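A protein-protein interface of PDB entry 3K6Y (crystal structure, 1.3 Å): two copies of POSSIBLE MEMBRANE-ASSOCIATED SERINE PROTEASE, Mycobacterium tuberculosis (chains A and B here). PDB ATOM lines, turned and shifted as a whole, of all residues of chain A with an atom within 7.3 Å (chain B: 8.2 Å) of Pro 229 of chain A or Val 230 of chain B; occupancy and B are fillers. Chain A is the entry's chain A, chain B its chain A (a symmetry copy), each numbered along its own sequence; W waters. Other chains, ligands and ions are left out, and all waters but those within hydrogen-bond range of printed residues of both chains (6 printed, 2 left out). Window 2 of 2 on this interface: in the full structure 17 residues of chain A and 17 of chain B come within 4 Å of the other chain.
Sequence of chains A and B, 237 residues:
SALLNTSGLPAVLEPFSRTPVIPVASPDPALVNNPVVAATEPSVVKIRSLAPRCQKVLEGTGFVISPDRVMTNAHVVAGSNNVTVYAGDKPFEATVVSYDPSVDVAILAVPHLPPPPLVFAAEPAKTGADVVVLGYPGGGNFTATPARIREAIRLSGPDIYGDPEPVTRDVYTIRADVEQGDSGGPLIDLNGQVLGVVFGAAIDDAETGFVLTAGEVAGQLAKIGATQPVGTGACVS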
ATOM      1  N   THR A  95       9.096  -7.205 -12.777  1.00  0.00           N
ATOM      2  CA  THR A  95       9.571  -5.845 -13.042  1.00  0.00           C
ATOM      3  C   THR A  95      11.024  -5.777 -12.586  1.00  0.00           C
ATOM      4  O   THR A  95      11.343  -6.226 -11.488  1.00  0.00           O
ATOM      5  CB  THR A  95       8.714  -4.797 -12.233  1.00  0.00           C
ATOM      6  OG1 THR A  95       7.354  -4.912 -12.671  1.00  0.00           O
ATOM      7  CG2 THR A  95       9.188  -3.388 -12.513  1.00  0.00           C
ATOM      8  N   VAL A  96      11.893  -5.179 -13.395  1.00  0.00           N
ATOM      9  CA  VAL A  96      13.281  -4.988 -12.982  1.00  0.00           C
ATOM     10  C   VAL A  96      13.321  -3.710 -12.116  1.00  0.00           C
ATOM     11  O   VAL A  96      13.131  -2.606 -12.627  1.00  0.00           O
ATOM     12  CB  VAL A  96      14.211  -4.830 -14.201  1.00  0.00           C
ATOM     13  CG1 VAL A  96      15.632  -4.672 -13.733  1.00  0.00           C
ATOM     14  CG2 VAL A  96      14.084  -6.034 -15.147  1.00  0.00           C
ATOM     15  N   VAL A  97      13.554  -3.858 -10.812  1.00  0.00           N
ATOM     16  CA  VAL A  97      13.534  -2.712  -9.912  1.00  0.00           C
ATOM     17  C   VAL A  97      14.905  -2.275  -9.443  1.00  0.00           C
ATOM     18  O   VAL A  97      15.052  -1.179  -8.893  1.00  0.00           O
ATOM     19  CB  VAL A  97      12.583  -2.929  -8.692  1.00  0.00           C
ATOM     20  CG1 VAL A  97      11.165  -3.147  -9.182  1.00  0.00           C
ATOM     21  CG2 VAL A  97      13.045  -4.083  -7.806  1.00  0.00           C
ATOM     22  N   SER A  98      15.917  -3.109  -9.678  1.00  0.00           N
ATOM     23  CA  SER A  98      17.307  -2.726  -9.437  1.00  0.00           C
ATOM     24  C   SER A  98      18.132  -3.423 -10.502  1.00  0.00           C
ATOM     25  O   SER A  98      17.883  -4.576 -10.838  1.00  0.00           O
ATOM     26  CB  SER A  98      17.749  -3.126  -8.028  1.00  0.00           C
ATOM     27  OG  SER A  98      19.102  -2.812  -7.794  1.00  0.00           O
ATOM     28  N   LYS A 223      18.446  -1.697  -2.256  1.00  0.00           N
ATOM     29  CA  LYS A 223      17.420  -1.236  -3.172  1.00  0.00           C
ATOM     30  C   LYS A 223      16.283  -2.223  -3.265  1.00  0.00           C
ATOM     31  O   LYS A 223      15.452  -2.077  -4.133  1.00  0.00           O
ATOM     32  CB  LYS A 223      17.981  -0.975  -4.576  1.00  0.00           C
ATOM     33  CG  LYS A 223      17.077  -0.098  -5.442  1.00  0.00           C
ATOM     34  CD  LYS A 223      17.850   0.612  -6.549  1.00  0.00           C
ATOM     35  CE  LYS A 223      16.883   1.330  -7.484  1.00  0.00           C
ATOM     36  NZ  LYS A 223      17.624   2.112  -8.534  1.00  0.00           N
ATOM     37  N   ALA A 226      12.630  -1.060  -3.772  1.00  0.00           N
ATOM     38  CA  ALA A 226      12.205  -0.391  -4.989  1.00  0.00           C
ATOM     39  C   ALA A 226      11.011  -1.087  -5.637  1.00  0.00           C
ATOM     40  O   ALA A 226      10.823  -2.309  -5.545  1.00  0.00           O
ATOM     41  CB  ALA A 226      13.343  -0.321  -5.952  1.00  0.00           C
ATOM     42  N   THR A 227      10.191  -0.272  -6.278  1.00  0.00           N
ATOM     43  CA  THR A 227       8.994  -0.748  -6.919  1.00  0.00           C
ATOM     44  C   THR A 227       8.871  -0.328  -8.386  1.00  0.00           C
ATOM     45  O   THR A 227       8.201  -0.996  -9.156  1.00  0.00           O
ATOM     46  CB  THR A 227       7.732  -0.246  -6.181  1.00  0.00           C
ATOM     47  OG1 THR A 227       7.814   1.170  -6.004  1.00  0.00           O
ATOM     48  CG2 THR A 227       7.586  -0.911  -4.806  1.00  0.00           C
ATOM     49  N   GLN A 228       9.557   0.746  -8.780  1.00  0.00           N
ATOM     50  CA  GLN A 228       9.419   1.271 -10.140  1.00  0.00           C
ATOM     51  C   GLN A 228      10.410   0.619 -11.086  1.00  0.00           C
ATOM     52  O   GLN A 228      11.506   0.266 -10.673  1.00  0.00           O
ATOM     53  CB  GLN A 228       9.638   2.781 -10.116  1.00  0.00           C
ATOM     54  CG  GLN A 228       8.638   3.516  -9.268  1.00  0.00           C
ATOM     55  CD  GLN A 228       7.242   3.127  -9.611  1.00  0.00           C
ATOM     56  OE1 GLN A 228       6.816   3.223 -10.773  1.00  0.00           O
ATOM     57  NE2 GLN A 228       6.507   2.632  -8.613  1.00  0.00           N
ATOM     58  N   PRO A 229      10.056   0.467 -12.364  1.00  0.00           N
ATOM     59  CA  PRO A 229      11.033  -0.136 -13.280  1.00  0.00           C
ATOM     60  C   PRO A 229      12.235   0.758 -13.542  1.00  0.00           C
ATOM     61  O   PRO A 229      12.097   1.976 -13.703  1.00  0.00           O
ATOM     62  CB  PRO A 229      10.247  -0.329 -14.579  1.00  0.00           C
ATOM     63  CG  PRO A 229       9.121   0.646 -14.502  1.00  0.00           C
ATOM     64  CD  PRO A 229       8.775   0.793 -13.025  1.00  0.00           C
ATOM     65  N   VAL A 230      13.403   0.138 -13.628  1.00  0.00           N
ATOM     66  CA  VAL A 230      14.618   0.854 -14.013  1.00  0.00           C
ATOM     67  C   VAL A 230      14.964   0.283 -15.415  1.00  0.00           C
ATOM     68  O   VAL A 230      14.487  -0.797 -15.784  1.00  0.00           O
ATOM     69  CB  VAL A 230      15.741   0.668 -12.947  1.00  0.00           C
ATOM     70  CG1 VAL A 230      15.273   1.207 -11.594  1.00  0.00           C
ATOM     71  CG2 VAL A 230      16.193  -0.794 -12.822  1.00  0.00           C
ATOM     72  N   GLY A 231      15.782   0.946 -16.184  1.00  0.00           N
ATOM     73  CA  GLY A 231      16.042   0.315 -17.492  1.00  0.00           C
ATOM     74  C   GLY A 231      16.906  -0.939 -17.393  1.00  0.00           C
ATOM     75  O   GLY A 231      17.490  -1.239 -16.337  1.00  0.00           O
ATOM     76  N   VAL B  77      23.562  11.765 -21.231  1.00  0.00           N
ATOM     77  CA  VAL B  77      23.705  11.247 -19.879  1.00  0.00           C
ATOM     78  C   VAL B  77      24.096   9.768 -19.835  1.00  0.00           C
ATOM     79  O   VAL B  77      24.277   9.223 -18.746  1.00  0.00           O
ATOM     80  CB  VAL B  77      22.391  11.479 -19.032  1.00  0.00           C
ATOM     81  CG1 VAL B  77      22.078  12.965 -18.930  1.00  0.00           C
ATOM     82  CG2 VAL B  77      21.195  10.709 -19.609  1.00  0.00           C
ATOM     83  N   SER B  80      26.470   7.764 -17.214  1.00  0.00           N
ATOM     84  CA  SER B  80      26.829   8.653 -16.131  1.00  0.00           C
ATOM     85  C   SER B  80      26.276   8.198 -14.800  1.00  0.00           C
ATOM     86  O   SER B  80      25.338   7.399 -14.737  1.00  0.00           O
ATOM     87  CB  SER B  80      26.301  10.057 -16.406  1.00  0.00           C
ATOM     88  OG  SER B  80      24.886  10.141 -16.334  1.00  0.00           O
ATOM     89  N   THR B  95      17.673  14.338 -11.542  1.00  0.00           N
ATOM     90  CA  THR B  95      17.453  12.890 -11.517  1.00  0.00           C
ATOM     91  C   THR B  95      17.007  12.475 -12.914  1.00  0.00           C
ATOM     92  O   THR B  95      16.134  13.115 -13.493  1.00  0.00           O
ATOM     93  CB  THR B  95      16.329  12.525 -10.473  1.00  0.00           C
ATOM     94  OG1 THR B  95      16.774  12.955  -9.179  1.00  0.00           O
ATOM     95  CG2 THR B  95      16.106  11.029 -10.428  1.00  0.00           C
ATOM     96  N   VAL B  96      17.563  11.387 -13.436  1.00  0.00           N
ATOM     97  CA  VAL B  96      17.114  10.872 -14.727  1.00  0.00           C
ATOM     98  C   VAL B  96      15.860  10.012 -14.459  1.00  0.00           C
ATOM     99  O   VAL B  96      15.956   8.941 -13.860  1.00  0.00           O
ATOM    100  CB  VAL B  96      18.206  10.017 -15.399  1.00  0.00           C
ATOM    101  CG1 VAL B  96      17.718   9.537 -16.739  1.00  0.00           C
ATOM    102  CG2 VAL B  96      19.511  10.814 -15.554  1.00  0.00           C
ATOM    103  N   VAL B  97      14.689  10.483 -14.884  1.00  0.00           N
ATOM    104  CA  VAL B  97      13.448   9.771 -14.606  1.00  0.00           C
ATOM    105  C   VAL B  97      12.861   9.064 -15.809  1.00  0.00           C
ATOM    106  O   VAL B  97      11.967   8.226 -15.660  1.00  0.00           O
ATOM    107  CB  VAL B  97      12.374  10.686 -13.935  1.00  0.00           C
ATOM    108  CG1 VAL B  97      12.905  11.210 -12.614  1.00  0.00           C
ATOM    109  CG2 VAL B  97      11.944  11.829 -14.849  1.00  0.00           C
ATOM    110  N   SER B  98      13.375   9.373 -16.999  1.00  0.00           N
ATOM    111  CA  SER B  98      13.021   8.632 -18.210  1.00  0.00           C
ATOM    112  C   SER B  98      14.264   8.617 -19.078  1.00  0.00           C
ATOM    113  O   SER B  98      14.977   9.610 -19.175  1.00  0.00           O
ATOM    114  CB  SER B  98      11.839   9.287 -18.927  1.00  0.00           C
ATOM    115  OG  SER B  98      11.516   8.619 -20.124  1.00  0.00           O
ATOM    116  N   TYR B  99      14.518   7.476 -19.699  1.00  0.00           N
ATOM    117  CA  TYR B  99      15.730   7.268 -20.465  1.00  0.00           C
ATOM    118  C   TYR B  99      15.392   6.274 -21.563  1.00  0.00           C
ATOM    119  O   TYR B  99      15.028   5.126 -21.277  1.00  0.00           O
ATOM    120  CB  TYR B  99      16.854   6.758 -19.552  1.00  0.00           C
ATOM    121  CG  TYR B  99      18.164   6.514 -20.266  1.00  0.00           C
ATOM    122  CD1 TYR B  99      19.111   7.527 -20.418  1.00  0.00           C
ATOM    123  CD2 TYR B  99      18.463   5.256 -20.775  1.00  0.00           C
ATOM    124  CE1 TYR B  99      20.312   7.283 -21.069  1.00  0.00           C
ATOM    125  CE2 TYR B  99      19.654   5.016 -21.434  1.00  0.00           C
ATOM    126  CZ  TYR B  99      20.560   6.032 -21.581  1.00  0.00           C
ATOM    127  OH  TYR B  99      21.737   5.783 -22.234  1.00  0.00           O
ATOM    128  N   ASP B 100      15.528   6.696 -22.819  1.00  0.00           N
ATOM    129  CA  ASP B 100      15.158   5.864 -23.964  1.00  0.00           C
ATOM    130  C   ASP B 100      16.295   5.945 -24.991  1.00  0.00           C
ATOM    131  O   ASP B 100      16.447   6.929 -25.705  1.00  0.00           O
ATOM    132  CB  ASP B 100      13.841   6.341 -24.577  1.00  0.00           C
ATOM    133  CG  ASP B 100      13.355   5.447 -25.698  1.00  0.00           C
ATOM    134  OD1 ASP B 100      14.198   4.847 -26.397  1.00  0.00           O
ATOM    135  OD2 ASP B 100      12.116   5.379 -25.898  1.00  0.00           O
ATOM    136  N   VAL B 105      16.302   9.929 -26.047  1.00  0.00           N
ATOM    137  CA  VAL B 105      15.769  11.039 -25.252  1.00  0.00           C
ATOM    138  C   VAL B 105      15.828  10.665 -23.788  1.00  0.00           C
ATOM    139  O   VAL B 105      15.576   9.509 -23.439  1.00  0.00           O
ATOM    140  CB  VAL B 105      14.305  11.353 -25.626  1.00  0.00           C
ATOM    141  CG1 VAL B 105      13.685  12.397 -24.670  1.00  0.00           C
ATOM    142  CG2 VAL B 105      14.224  11.853 -27.044  1.00  0.00           C
ATOM    143  N   ALA B 106      16.175  11.638 -22.951  1.00  0.00           N
ATOM    144  CA  ALA B 106      16.066  11.495 -21.506  1.00  0.00           C
ATOM    145  C   ALA B 106      15.261  12.659 -20.968  1.00  0.00           C
ATOM    146  O   ALA B 106      15.314  13.777 -21.511  1.00  0.00           O
ATOM    147  CB  ALA B 106      17.458  11.446 -20.833  1.00  0.00           C
ATOM    148  N   ILE B 107      14.521  12.402 -19.889  1.00  0.00           N
ATOM    149  CA  ILE B 107      13.848  13.478 -19.163  1.00  0.00           C
ATOM    150  C   ILE B 107      14.427  13.505 -17.763  1.00  0.00           C
ATOM    151  O   ILE B 107      14.575  12.451 -17.109  1.00  0.00           O
ATOM    152  CB  ILE B 107      12.306  13.284 -19.117  1.00  0.00           C
ATOM    153  CG1 ILE B 107      11.741  13.336 -20.546  1.00  0.00           C
ATOM    154  CG2 ILE B 107      11.652  14.362 -18.227  1.00  0.00           C
ATOM    155  CD1 ILE B 107      10.231  13.038 -20.662  1.00  0.00           C
ATOM    156  N   LYS B 223       5.931   9.654 -19.828  1.00  0.00           N
ATOM    157  CA  LYS B 223       6.627   9.307 -18.603  1.00  0.00           C
ATOM    158  C   LYS B 223       7.052  10.539 -17.845  1.00  0.00           C
ATOM    159  O   LYS B 223       7.813  10.418 -16.910  1.00  0.00           O
ATOM    160  CB  LYS B 223       7.856   8.429 -18.873  1.00  0.00           C
ATOM    161  CG  LYS B 223       8.362   7.689 -17.635  1.00  0.00           C
ATOM    162  CD  LYS B 223       9.159   6.438 -17.994  1.00  0.00           C
ATOM    163  CE  LYS B 223       9.785   5.838 -16.740  1.00  0.00           C
ATOM    164  NZ  LYS B 223      10.501   4.553 -17.054  1.00  0.00           N
ATOM    165  N   ALA B 226       7.112  10.614 -13.979  1.00  0.00           N
ATOM    166  CA  ALA B 226       8.021   9.779 -13.214  1.00  0.00           C
ATOM    167  C   ALA B 226       8.864  10.595 -12.239  1.00  0.00           C
ATOM    168  O   ALA B 226       9.201  11.766 -12.469  1.00  0.00           O
ATOM    169  CB  ALA B 226       8.903   9.012 -14.141  1.00  0.00           C
ATOM    170  N   THR B 227       9.182   9.953 -11.128  1.00  0.00           N
ATOM    171  CA  THR B 227       9.944  10.580 -10.079  1.00  0.00           C
ATOM    172  C   THR B 227      11.173   9.778  -9.648  1.00  0.00           C
ATOM    173  O   THR B 227      12.125  10.349  -9.141  1.00  0.00           O
ATOM    174  CB  THR B 227       9.072  10.813  -8.824  1.00  0.00           C
ATOM    175  OG1 THR B 227       8.417   9.594  -8.465  1.00  0.00           O
ATOM    176  CG2 THR B 227       8.012  11.893  -9.071  1.00  0.00           C
ATOM    177  N   GLN B 228      11.175   8.467  -9.896  1.00  0.00           N
ATOM    178  CA  GLN B 228      12.269   7.613  -9.430  1.00  0.00           C
ATOM    179  C   GLN B 228      13.385   7.539 -10.453  1.00  0.00           C
ATOM    180  O   GLN B 228      13.124   7.604 -11.647  1.00  0.00           O
ATOM    181  CB  GLN B 228      11.725   6.215  -9.149  1.00  0.00           C
ATOM    182  CG  GLN B 228      10.671   6.188  -8.078  1.00  0.00           C
ATOM    183  CD  GLN B 228      11.122   6.902  -6.852  1.00  0.00           C
ATOM    184  OE1 GLN B 228      12.177   6.589  -6.278  1.00  0.00           O
ATOM    185  NE2 GLN B 228      10.354   7.915  -6.445  1.00  0.00           N
ATOM    186  N   PRO B 229      14.635   7.382 -10.013  1.00  0.00           N
ATOM    187  CA  PRO B 229      15.707   7.279 -11.013  1.00  0.00           C
ATOM    188  C   PRO B 229      15.648   5.990 -11.819  1.00  0.00           C
ATOM    189  O   PRO B 229      15.378   4.913 -11.277  1.00  0.00           O
ATOM    190  CB  PRO B 229      16.990   7.301 -10.178  1.00  0.00           C
ATOM    191  CG  PRO B 229      16.576   6.856  -8.815  1.00  0.00           C
ATOM    192  CD  PRO B 229      15.138   7.324  -8.626  1.00  0.00           C
ATOM    193  N   VAL B 230      15.948   6.104 -13.105  1.00  0.00           N
ATOM    194  CA  VAL B 230      16.066   4.930 -13.966  1.00  0.00           C
ATOM    195  C   VAL B 230      17.580   4.860 -14.303  1.00  0.00           C
ATOM    196  O   VAL B 230      18.298   5.857 -14.159  1.00  0.00           O
ATOM    197  CB  VAL B 230      15.135   5.050 -15.212  1.00  0.00           C
ATOM    198  CG1 VAL B 230      13.677   5.175 -14.764  1.00  0.00           C
ATOM    199  CG2 VAL B 230      15.525   6.222 -16.123  1.00  0.00           C
ATOM    200  N   GLY B 231      18.076   3.744 -14.762  1.00  0.00           N
ATOM    201  CA  GLY B 231      19.522   3.787 -15.049  1.00  0.00           C
ATOM    202  C   GLY B 231      19.866   4.625 -16.277  1.00  0.00           C
ATOM    203  O   GLY B 231      18.981   5.028 -17.052  1.00  0.00           O
ATOM    204  N   THR B 232      21.161   4.815 -16.499  1.00  0.00           N
ATOM    205  CA  THR B 232      21.657   5.505 -17.685  1.00  0.00           C
ATOM    206  C   THR B 232      22.398   4.575 -18.630  1.00  0.00           C
ATOM    207  O   THR B 232      23.110   5.034 -19.528  1.00  0.00           O
ATOM    208  CB  THR B 232      22.550   6.668 -17.312  1.00  0.00           C
ATOM    209  OG1 THR B 232      23.544   6.165 -16.421  1.00  0.00           O
ATOM    210  CG2 THR B 232      21.738   7.793 -16.672  1.00  0.00           C
ATOM    211  N   GLY B 233      22.215   3.268 -18.484  1.00  0.00           N
ATOM    212  CA  GLY B 233      22.698   2.331 -19.487  1.00  0.00           C
ATOM    213  C   GLY B 233      24.211   2.258 -19.631  1.00  0.00           C
ATOM    214  O   GLY B 233      24.980   2.501 -18.692  1.00  0.00           O
HETATM  215  O   HOH W   1      18.948   0.672 -14.996  1.00  0.00           O
HETATM  216  O   HOH W   2      14.773   3.530  -9.038  1.00  0.00           O
HETATM  217  O   HOH W   3      10.473   4.127 -13.858  1.00  0.00           O
HETATM  218  O   HOH W   4      17.068   3.274 -17.968  1.00  0.00           O
HETATM  219  O   HOH W   5      17.900   3.567 -11.045  1.00  0.00           O
HETATM  220  O   HOH W   6      12.356   2.365 -16.534  1.00  0.00           O
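The backbone NH of Val 230 of chain A is in hydrogen-bond range of the backbone carbonyl oxygen of Val 96 of chain A (2.9 Å).
The side-chain amide nitrogen (NE2) of Gln 228 of chain A is in hydrogen-bond range of the side-chain hydroxyl (OG1) of Thr 227 of chain A, at 3.3 Å.
The backbone carbonyl oxygen (O) of Val 96 of chain B sits at hydrogen-bond distance from the backbone NH (N) of Val 230 of chain B (2.9 Å).
The side-chain hydroxyl of Thr 227 of chain B lies within hydrogen-bond range of the side-chain amide nitrogen of Gln 228 of chain B, 3.3 Å away.
Among the printed residues, pairs that only touch across the chains: Gln 228 of chain A with Gln 228 of chain B, Val 230 of chain A with Pro 229 of chain B, Pro 229 of chain A with Val 230 of chain B and Gly 231 of chain A with Gly 231 of chain B.
Of the printed residues of chain B, Pro 229 of chain A touches Val 230 (3.7 Å).
Of chain A, only Pro 229 (3.7 Å) comes within 4 Å of Val 230 of chain B.
Of the printed residues of chain A, Gly 231 of chain B touches Gly 231 (3.9 Å).
Of the printed residues of chain B, Val 230 of chain A touches Pro 229.
Of the printed residues of chain B, Gln 228 of chain A touches Gln 228 (3.6 Å).
Of the printed residues of chain A, Pro 229 of chain B touches Val 230 (3.7 Å).
Ser 98 of chain B touches none of the printed residues of chain A.
The nearest printed residue of chain A that does not touch Gln 228 of chain B is Pro 229 of chain A (6.1 Å).
Along chain A the printed residues that touch a printed residue of chain B span positions 228 to 231.
Of the 20 printed residues of chain B, 4 touch a printed residue of chain A.
Printed residues of chain B that touch a printed residue of chain A: Gln 228, Pro 229, Val 230 and Gly 231.
Gln 228 of chain B touches its own counterpart, Gln 228 of chain A.
Pro 229 of chain A touches Val 230 of chain B, and with the chains exchanged Val 230 of chain A touches Pro 229 of chain B.
Gly 231 of chain A touches its own counterpart, Gly 231 of chain B.
Positions printed for both chains: 95, 96, 97, 98, 223, 226, 227, 228, 229, 230 and 231.
Of the 4 pairs that touch across the chains among the printed residues, 4 have their exchanged pair printed and touching as well.
Water W3 lies within hydrogen-bond range of the backbone carbonyl oxygen (O) of Pro 229 of chain A (2.7 Å) and the side-chain amino group (NZ) of Lys 223 of chain B (3.2 Å).
Water W2 bridges O of Pro 229 of chain B (2.7 Å) and NZ of Lys 223 of chain A (3.2 Å).
Water W1 lies within hydrogen-bond range of O of Gly 231 of chain A and N of Gly 231 of chain B.
Water W4 bridges O of Gly 231 of chain B and N of Gly 231 of chain A.
Water W5 lies within hydrogen-bond range of the backbone carbonyl oxygen of Pro 229 of chain B (2.9 Å) and the side-chain amino group of Lys 223 of chain A (2.9 Å).
Water W6 bridges the backbone carbonyl oxygen of Pro 229 of chain A (2.9 Å) and the side-chain amino group of Lys 223 of chain B (2.9 Å).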
